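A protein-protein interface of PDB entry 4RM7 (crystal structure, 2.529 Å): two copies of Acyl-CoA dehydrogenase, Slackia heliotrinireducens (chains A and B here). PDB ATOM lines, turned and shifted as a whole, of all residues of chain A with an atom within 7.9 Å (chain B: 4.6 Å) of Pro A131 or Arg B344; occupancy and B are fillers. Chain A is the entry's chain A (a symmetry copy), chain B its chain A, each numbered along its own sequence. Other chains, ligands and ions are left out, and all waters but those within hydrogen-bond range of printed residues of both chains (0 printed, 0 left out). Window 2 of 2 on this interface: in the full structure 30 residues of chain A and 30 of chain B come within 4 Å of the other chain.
The side-chain sulfur of Met A158 lies within hydrogen-bond range of the guanidinium group of Arg B344 (3.3 Å).
The backbone carbonyl oxygen (O) of Ser A129 sits at hydrogen-bond distance from the backbone NH (N) of Met A158 (2.8 Å). The side-chain carboxylate (OE2) of Glu A202 lies within hydrogen-bond range of the side-chain hydroxyl (OG1) of Thr A214 (3.1 Å).
Arg B344 touches Pro A131 (NH2 to O, 3.9 Å). Phe A159 touches Gly B343. Arg B344 touches Phe A159 (N to CZ, 3.7 Å). Ile B347 touches Glu A202. Gly B342 touches Phe A364. Phe A364 touches Gly B343 (CD1 to N, 3.8 Å). Phe A364 touches Tyr B346.
Pro A131 touches just one residue of chain B: Arg B344 (3.9 Å). Thr A142 touches none of the printed residues of chain B. Printed residues of chain B within 4 Å of Phe A364: Gly B342, Gly B343 and Tyr B346. Arg B271 touches none of the printed residues of chain A. Of the printed residues of chain A, Gly B342 touches Phe A364 (3.2 Å). Gly B343 touches two residues of chain A. The nearest printed residue of chain B that does not touch Phe A159 is Ile B347 (5.2 Å).
Of the 9 printed residues of chain B, 5 touch a printed residue of chain A. Printed residues of chain B that touch a printed residue of chain A: Gly B342, Gly B343, Arg B344, Tyr B346 and Ile B347. Hydrophobic or aromatic side chains of chain B that line the printed part of chain A: Tyr B346 and Ile B347. Along chain B the printed residues that touch a printed residue of chain A span positions 342 to 347. Of the 17 printed residues of chain A, 5 touch a printed residue of chain B. Printed residues of chain A that touch a printed residue of chain B: Pro A131, Met A158, Phe A159, Glu A202 and Phe A364. Among the printed residues, 8 pairs touch across the chains.
No position is printed for both chains. Of the 8 pairs that touch across the chains among the printed residues, none has its exchanged pair printed and touching as well.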
ATOM      1  N   ILE A 128      18.090 -10.691   3.318  1.00  0.00           N
ATOM      2  CA  ILE A 128      17.761 -11.780   2.401  1.00  0.00           C
ATOM      3  C   ILE A 128      16.303 -12.256   2.441  1.00  0.00           C
ATOM      4  O   ILE A 128      15.668 -12.403   1.397  1.00  0.00           O
ATOM      5  CB  ILE A 128      18.618 -12.997   2.677  1.00  0.00           C
ATOM      6  CG1 ILE A 128      20.078 -12.616   2.862  1.00  0.00           C
ATOM      7  CG2 ILE A 128      18.491 -13.985   1.537  1.00  0.00           C
ATOM      8  CD1 ILE A 128      20.918 -13.823   3.253  1.00  0.00           C
ATOM      9  N   SER A 129      15.780 -12.531   3.634  1.00  0.00           N
ATOM     10  CA  SER A 129      14.426 -13.085   3.760  1.00  0.00           C
ATOM     11  C   SER A 129      13.333 -12.172   3.210  1.00  0.00           C
ATOM     12  O   SER A 129      13.386 -10.960   3.388  1.00  0.00           O
ATOM     13  CB  SER A 129      14.121 -13.393   5.224  1.00  0.00           C
ATOM     14  OG  SER A 129      15.163 -14.157   5.816  1.00  0.00           O
ATOM     15  N   GLU A 130      12.330 -12.757   2.562  1.00  0.00           N
ATOM     16  CA  GLU A 130      11.177 -12.001   2.076  1.00  0.00           C
ATOM     17  C   GLU A 130       9.878 -12.593   2.615  1.00  0.00           C
ATOM     18  O   GLU A 130       9.786 -13.806   2.829  1.00  0.00           O
ATOM     19  CB  GLU A 130      11.134 -11.984   0.548  1.00  0.00           C
ATOM     20  CG  GLU A 130      12.478 -11.881  -0.105  1.00  0.00           C
ATOM     21  CD  GLU A 130      12.454 -11.005  -1.332  1.00  0.00           C
ATOM     22  OE1 GLU A 130      13.528 -10.809  -1.930  1.00  0.00           O
ATOM     23  OE2 GLU A 130      11.368 -10.505  -1.697  1.00  0.00           O
ATOM     24  N   PRO A 131       8.858 -11.739   2.814  1.00  0.00           N
ATOM     25  CA  PRO A 131       7.572 -12.156   3.388  1.00  0.00           C
ATOM     26  C   PRO A 131       6.848 -13.270   2.623  1.00  0.00           C
ATOM     27  O   PRO A 131       6.190 -14.097   3.254  1.00  0.00           O
ATOM     28  CB  PRO A 131       6.738 -10.863   3.351  1.00  0.00           C
ATOM     29  CG  PRO A 131       7.447  -9.954   2.400  1.00  0.00           C
ATOM     30  CD  PRO A 131       8.887 -10.292   2.534  1.00  0.00           C
ATOM     31  N   GLU A 132       6.983 -13.285   1.299  1.00  0.00           N
ATOM     32  CA  GLU A 132       6.159 -14.128   0.435  1.00  0.00           C
ATOM     33  C   GLU A 132       4.681 -13.822   0.647  1.00  0.00           C
ATOM     34  O   GLU A 132       3.832 -14.703   0.516  1.00  0.00           O
ATOM     35  CB  GLU A 132       6.427 -15.608   0.687  1.00  0.00           C
ATOM     36  CG  GLU A 132       7.884 -15.991   0.614  1.00  0.00           C
ATOM     37  CD  GLU A 132       8.110 -17.418   1.052  1.00  0.00           C
ATOM     38  OE1 GLU A 132       7.240 -17.961   1.771  1.00  0.00           O
ATOM     39  OE2 GLU A 132       9.149 -18.001   0.677  1.00  0.00           O
ATOM     40  N   MET A 140      11.336 -15.515  -4.028  1.00  0.00           N
ATOM     41  CA  MET A 140      12.002 -14.228  -3.837  1.00  0.00           C
ATOM     42  C   MET A 140      11.547 -13.179  -4.861  1.00  0.00           C
ATOM     43  O   MET A 140      11.594 -13.421  -6.066  1.00  0.00           O
ATOM     44  CB  MET A 140      13.521 -14.399  -3.912  1.00  0.00           C
ATOM     45  CG  MET A 140      14.272 -13.097  -4.175  1.00  0.00           C
ATOM     46  SD  MET A 140      16.213 -13.223  -4.020  1.00  0.00           S
ATOM     47  CE  MET A 140      16.314 -13.977  -2.198  1.00  0.00           C
ATOM     48  N   ARG A 141      11.139 -12.007  -4.374  1.00  0.00           N
ATOM     49  CA  ARG A 141      10.519 -11.000  -5.227  1.00  0.00           C
ATOM     50  C   ARG A 141      11.237  -9.638  -5.260  1.00  0.00           C
ATOM     51  O   ARG A 141      10.703  -8.679  -5.816  1.00  0.00           O
ATOM     52  CB  ARG A 141       9.055 -10.802  -4.802  1.00  0.00           C
ATOM     53  CG  ARG A 141       8.163 -12.039  -4.990  1.00  0.00           C
ATOM     54  CD  ARG A 141       8.423 -12.729  -6.344  1.00  0.00           C
ATOM     55  NE  ARG A 141       7.558 -13.887  -6.611  1.00  0.00           N
ATOM     56  CZ  ARG A 141       7.766 -15.122  -6.149  1.00  0.00           C
ATOM     57  NH1 ARG A 141       8.806 -15.387  -5.363  1.00  0.00           N
ATOM     58  NH2 ARG A 141       6.920 -16.098  -6.462  1.00  0.00           N
ATOM     59  N   THR A 142      12.438  -9.547  -4.690  1.00  0.00           N
ATOM     60  CA  THR A 142      13.213  -8.300  -4.749  1.00  0.00           C
ATOM     61  C   THR A 142      14.015  -8.223  -6.044  1.00  0.00           C
ATOM     62  O   THR A 142      14.866  -9.068  -6.308  1.00  0.00           O
ATOM     63  CB  THR A 142      14.178  -8.145  -3.532  1.00  0.00           C
ATOM     64  OG1 THR A 142      13.420  -7.899  -2.344  1.00  0.00           O
ATOM     65  CG2 THR A 142      15.126  -6.978  -3.727  1.00  0.00           C
ATOM     66  N   GLY A 155      11.837  -4.081  -3.501  1.00  0.00           N
ATOM     67  CA  GLY A 155      11.651  -5.282  -2.718  1.00  0.00           C
ATOM     68  C   GLY A 155      11.550  -4.954  -1.244  1.00  0.00           C
ATOM     69  O   GLY A 155      11.697  -3.801  -0.843  1.00  0.00           O
ATOM     70  N   THR A 156      11.295  -5.980  -0.440  1.00  0.00           N
ATOM     71  CA  THR A 156      11.141  -5.843   0.998  1.00  0.00           C
ATOM     72  C   THR A 156      11.851  -6.993   1.686  1.00  0.00           C
ATOM     73  O   THR A 156      11.575  -8.162   1.412  1.00  0.00           O
ATOM     74  CB  THR A 156       9.669  -5.837   1.430  1.00  0.00           C
ATOM     75  OG1 THR A 156       9.071  -4.595   1.068  1.00  0.00           O
ATOM     76  CG2 THR A 156       9.552  -5.993   2.937  1.00  0.00           C
ATOM     77  N   LYS A 157      12.777  -6.663   2.573  1.00  0.00           N
ATOM     78  CA  LYS A 157      13.506  -7.685   3.282  1.00  0.00           C
ATOM     79  C   LYS A 157      13.036  -7.717   4.717  1.00  0.00           C
ATOM     80  O   LYS A 157      12.719  -6.688   5.306  1.00  0.00           O
ATOM     81  CB  LYS A 157      15.008  -7.442   3.188  1.00  0.00           C
ATOM     82  CG  LYS A 157      15.543  -7.577   1.791  1.00  0.00           C
ATOM     83  CD  LYS A 157      15.326  -8.972   1.215  1.00  0.00           C
ATOM     84  CE  LYS A 157      16.049  -9.103  -0.114  1.00  0.00           C
ATOM     85  NZ  LYS A 157      15.942 -10.459  -0.737  1.00  0.00           N
ATOM     86  N   MET A 158      12.983  -8.924   5.260  1.00  0.00           N
ATOM     87  CA  MET A 158      12.389  -9.189   6.561  1.00  0.00           C
ATOM     88  C   MET A 158      13.449  -9.716   7.507  1.00  0.00           C
ATOM     89  O   MET A 158      14.436 -10.301   7.067  1.00  0.00           O
ATOM     90  CB  MET A 158      11.257 -10.197   6.402  1.00  0.00           C
ATOM     91  CG  MET A 158      10.231 -10.196   7.504  1.00  0.00           C
ATOM     92  SD  MET A 158       8.444 -10.389   6.753  1.00  0.00           S
ATOM     93  CE  MET A 158       8.425  -8.736   5.715  1.00  0.00           C
ATOM     94  N   PHE A 159      13.256  -9.494   8.798  1.00  0.00           N
ATOM     95  CA  PHE A 159      14.159 -10.028   9.820  1.00  0.00           C
ATOM     96  C   PHE A 159      15.619  -9.642   9.550  1.00  0.00           C
ATOM     97  O   PHE A 159      16.511 -10.478   9.607  1.00  0.00           O
ATOM     98  CB  PHE A 159      14.015 -11.555   9.906  1.00  0.00           C
ATOM     99  CG  PHE A 159      12.581 -12.034   9.990  1.00  0.00           C
ATOM    100  CD1 PHE A 159      11.740 -11.589  10.999  1.00  0.00           C
ATOM    101  CD2 PHE A 159      12.078 -12.945   9.066  1.00  0.00           C
ATOM    102  CE1 PHE A 159      10.410 -12.039  11.084  1.00  0.00           C
ATOM    103  CE2 PHE A 159      10.753 -13.395   9.141  1.00  0.00           C
ATOM    104  CZ  PHE A 159       9.923 -12.946  10.151  1.00  0.00           C
ATOM    105  N   GLU A 202      11.473  -4.164  14.484  1.00  0.00           N
ATOM    106  CA  GLU A 202      10.518  -5.134  15.015  1.00  0.00           C
ATOM    107  C   GLU A 202      10.959  -5.604  16.396  1.00  0.00           C
ATOM    108  O   GLU A 202      11.938  -6.332  16.519  1.00  0.00           O
ATOM    109  CB  GLU A 202      10.386  -6.338  14.079  1.00  0.00           C
ATOM    110  CG  GLU A 202      10.052  -6.013  12.628  1.00  0.00           C
ATOM    111  CD  GLU A 202       8.602  -5.562  12.422  1.00  0.00           C
ATOM    112  OE1 GLU A 202       7.801  -5.624  13.386  1.00  0.00           O
ATOM    113  OE2 GLU A 202       8.267  -5.145  11.288  1.00  0.00           O
ATOM    114  N   THR A 214      12.317  -4.830   9.419  1.00  0.00           N
ATOM    115  CA  THR A 214      11.839  -4.965   8.053  1.00  0.00           C
ATOM    116  C   THR A 214      12.382  -3.777   7.273  1.00  0.00           C
ATOM    117  O   THR A 214      12.294  -2.634   7.730  1.00  0.00           O
ATOM    118  CB  THR A 214      10.295  -4.997   7.973  1.00  0.00           C
ATOM    119  OG1 THR A 214       9.787  -6.096   8.738  1.00  0.00           O
ATOM    120  CG2 THR A 214       9.833  -5.139   6.538  1.00  0.00           C
ATOM    121  N   VAL A 215      12.961  -4.038   6.109  1.00  0.00           N
ATOM    122  CA  VAL A 215      13.508  -2.965   5.297  1.00  0.00           C
ATOM    123  C   VAL A 215      12.877  -2.965   3.919  1.00  0.00           C
ATOM    124  O   VAL A 215      12.948  -3.958   3.197  1.00  0.00           O
ATOM    125  CB  VAL A 215      15.042  -3.080   5.154  1.00  0.00           C
ATOM    126  CG1 VAL A 215      15.563  -1.946   4.316  1.00  0.00           C
ATOM    127  CG2 VAL A 215      15.706  -3.072   6.520  1.00  0.00           C
ATOM    128  N   PHE A 364      12.126 -20.431  15.012  1.00  0.00           N
ATOM    129  CA  PHE A 364      11.864 -19.673  13.766  1.00  0.00           C
ATOM    130  C   PHE A 364      13.110 -19.320  12.973  1.00  0.00           C
ATOM    131  O   PHE A 364      13.053 -19.132  11.759  1.00  0.00           O
ATOM    132  CB  PHE A 364      11.146 -18.354  14.042  1.00  0.00           C
ATOM    133  CG  PHE A 364       9.840 -18.519  14.706  1.00  0.00           C
ATOM    134  CD1 PHE A 364       8.751 -18.973  13.998  1.00  0.00           C
ATOM    135  CD2 PHE A 364       9.689 -18.214  16.041  1.00  0.00           C
ATOM    136  CE1 PHE A 364       7.534 -19.116  14.613  1.00  0.00           C
ATOM    137  CE2 PHE A 364       8.476 -18.360  16.655  1.00  0.00           C
ATOM    138  CZ  PHE A 364       7.400 -18.810  15.947  1.00  0.00           C
ATOM    139  N   TRP B 267      -5.274 -16.295  10.418  1.00  0.00           N
ATOM    140  CA  TRP B 267      -4.049 -16.248   9.638  1.00  0.00           C
ATOM    141  C   TRP B 267      -4.056 -17.353   8.595  1.00  0.00           C
ATOM    142  O   TRP B 267      -3.742 -17.130   7.436  1.00  0.00           O
ATOM    143  CB  TRP B 267      -2.826 -16.398  10.540  1.00  0.00           C
ATOM    144  CG  TRP B 267      -1.526 -16.399   9.792  1.00  0.00           C
ATOM    145  CD1 TRP B 267      -0.914 -17.474   9.208  1.00  0.00           C
ATOM    146  CD2 TRP B 267      -0.672 -15.273   9.558  1.00  0.00           C
ATOM    147  NE1 TRP B 267       0.267 -17.083   8.619  1.00  0.00           N
ATOM    148  CE2 TRP B 267       0.438 -15.738   8.819  1.00  0.00           C
ATOM    149  CE3 TRP B 267      -0.745 -13.910   9.889  1.00  0.00           C
ATOM    150  CZ2 TRP B 267       1.468 -14.887   8.399  1.00  0.00           C
ATOM    151  CZ3 TRP B 267       0.280 -13.068   9.475  1.00  0.00           C
ATOM    152  CH2 TRP B 267       1.370 -13.560   8.738  1.00  0.00           C
ATOM    153  N   ARG B 271      -3.996 -15.966   5.006  1.00  0.00           N
ATOM    154  CA  ARG B 271      -2.686 -15.987   4.377  1.00  0.00           C
ATOM    155  C   ARG B 271      -2.463 -17.247   3.541  1.00  0.00           C
ATOM    156  O   ARG B 271      -3.227 -18.212   3.612  1.00  0.00           O
ATOM    157  CB  ARG B 271      -1.595 -15.835   5.438  1.00  0.00           C
ATOM    158  CG  ARG B 271      -1.901 -14.756   6.486  1.00  0.00           C
ATOM    159  CD  ARG B 271      -1.836 -13.350   5.938  1.00  0.00           C
ATOM    160  NE  ARG B 271      -0.484 -12.980   5.529  1.00  0.00           N
ATOM    161  CZ  ARG B 271      -0.129 -11.760   5.125  1.00  0.00           C
ATOM    162  NH1 ARG B 271      -1.027 -10.781   5.083  1.00  0.00           N
ATOM    163  NH2 ARG B 271       1.129 -11.515   4.767  1.00  0.00           N
ATOM    164  N   LEU B 341       1.649 -18.592  12.917  1.00  0.00           N
ATOM    165  CA  LEU B 341       1.794 -17.206  12.439  1.00  0.00           C
ATOM    166  C   LEU B 341       3.200 -16.929  11.913  1.00  0.00           C
ATOM    167  O   LEU B 341       3.422 -15.928  11.247  1.00  0.00           O
ATOM    168  CB  LEU B 341       1.473 -16.191  13.529  1.00  0.00           C
ATOM    169  CG  LEU B 341       0.132 -16.216  14.256  1.00  0.00           C
ATOM    170  CD1 LEU B 341       0.050 -15.040  15.182  1.00  0.00           C
ATOM    171  CD2 LEU B 341      -1.000 -16.145  13.322  1.00  0.00           C
ATOM    172  N   GLY B 342       4.140 -17.817  12.220  1.00  0.00           N
ATOM    173  CA  GLY B 342       5.481 -17.753  11.666  1.00  0.00           C
ATOM    174  C   GLY B 342       6.349 -16.767  12.423  1.00  0.00           C
ATOM    175  O   GLY B 342       6.061 -16.449  13.574  1.00  0.00           O
ATOM    176  N   GLY B 343       7.392 -16.270  11.759  1.00  0.00           N
ATOM    177  CA  GLY B 343       8.370 -15.377  12.363  1.00  0.00           C
ATOM    178  C   GLY B 343       7.789 -14.163  13.055  1.00  0.00           C
ATOM    179  O   GLY B 343       8.119 -13.896  14.209  1.00  0.00           O
ATOM    180  N   ARG B 344       6.940 -13.418  12.352  1.00  0.00           N
ATOM    181  CA  ARG B 344       6.177 -12.359  13.001  1.00  0.00           C
ATOM    182  C   ARG B 344       5.218 -13.021  13.966  1.00  0.00           C
ATOM    183  O   ARG B 344       4.723 -14.106  13.691  1.00  0.00           O
ATOM    184  CB  ARG B 344       5.434 -11.498  11.985  1.00  0.00           C
ATOM    185  CG  ARG B 344       4.827 -12.253  10.829  1.00  0.00           C
ATOM    186  CD  ARG B 344       4.560 -11.294   9.688  1.00  0.00           C
ATOM    187  NE  ARG B 344       4.063 -11.970   8.494  1.00  0.00           N
ATOM    188  CZ  ARG B 344       4.837 -12.547   7.577  1.00  0.00           C
ATOM    189  NH1 ARG B 344       6.154 -12.541   7.719  1.00  0.00           N
ATOM    190  NH2 ARG B 344       4.294 -13.135   6.519  1.00  0.00           N
ATOM    191  N   GLY B 345       4.959 -12.415  15.110  1.00  0.00           N
ATOM    192  CA  GLY B 345       4.243 -13.178  16.116  1.00  0.00           C
ATOM    193  C   GLY B 345       5.170 -13.884  17.106  1.00  0.00           C
ATOM    194  O   GLY B 345       4.715 -14.577  18.030  1.00  0.00           O
ATOM    195  N   TYR B 346       6.476 -13.727  16.889  1.00  0.00           N
ATOM    196  CA  TYR B 346       7.454 -13.799  17.973  1.00  0.00           C
ATOM    197  C   TYR B 346       7.806 -12.336  18.291  1.00  0.00           C
ATOM    198  O   TYR B 346       8.736 -12.024  19.047  1.00  0.00           O
ATOM    199  CB  TYR B 346       8.673 -14.630  17.566  1.00  0.00           C
ATOM    200  CG  TYR B 346       9.809 -14.675  18.572  1.00  0.00           C
ATOM    201  CD1 TYR B 346       9.707 -15.412  19.760  1.00  0.00           C
ATOM    202  CD2 TYR B 346      11.005 -13.996  18.314  1.00  0.00           C
ATOM    203  CE1 TYR B 346      10.772 -15.458  20.668  1.00  0.00           C
ATOM    204  CE2 TYR B 346      12.072 -14.024  19.212  1.00  0.00           C
ATOM    205  CZ  TYR B 346      11.960 -14.750  20.382  1.00  0.00           C
ATOM    206  OH  TYR B 346      13.047 -14.761  21.241  1.00  0.00           O
ATOM    207  N   ILE B 347       7.028 -11.446  17.679  1.00  0.00           N
ATOM    208  CA  ILE B 347       7.157 -10.007  17.852  1.00  0.00           C
ATOM    209  C   ILE B 347       6.249  -9.578  19.007  1.00  0.00           C
ATOM    210  O   ILE B 347       5.144 -10.093  19.159  1.00  0.00           O
ATOM    211  CB  ILE B 347       6.801  -9.260  16.539  1.00  0.00           C
ATOM    212  CG1 ILE B 347       7.628  -9.818  15.381  1.00  0.00           C
ATOM    213  CG2 ILE B 347       7.034  -7.771  16.659  1.00  0.00           C
ATOM    214  CD1 ILE B 347       7.257  -9.233  14.048  1.00  0.00           C
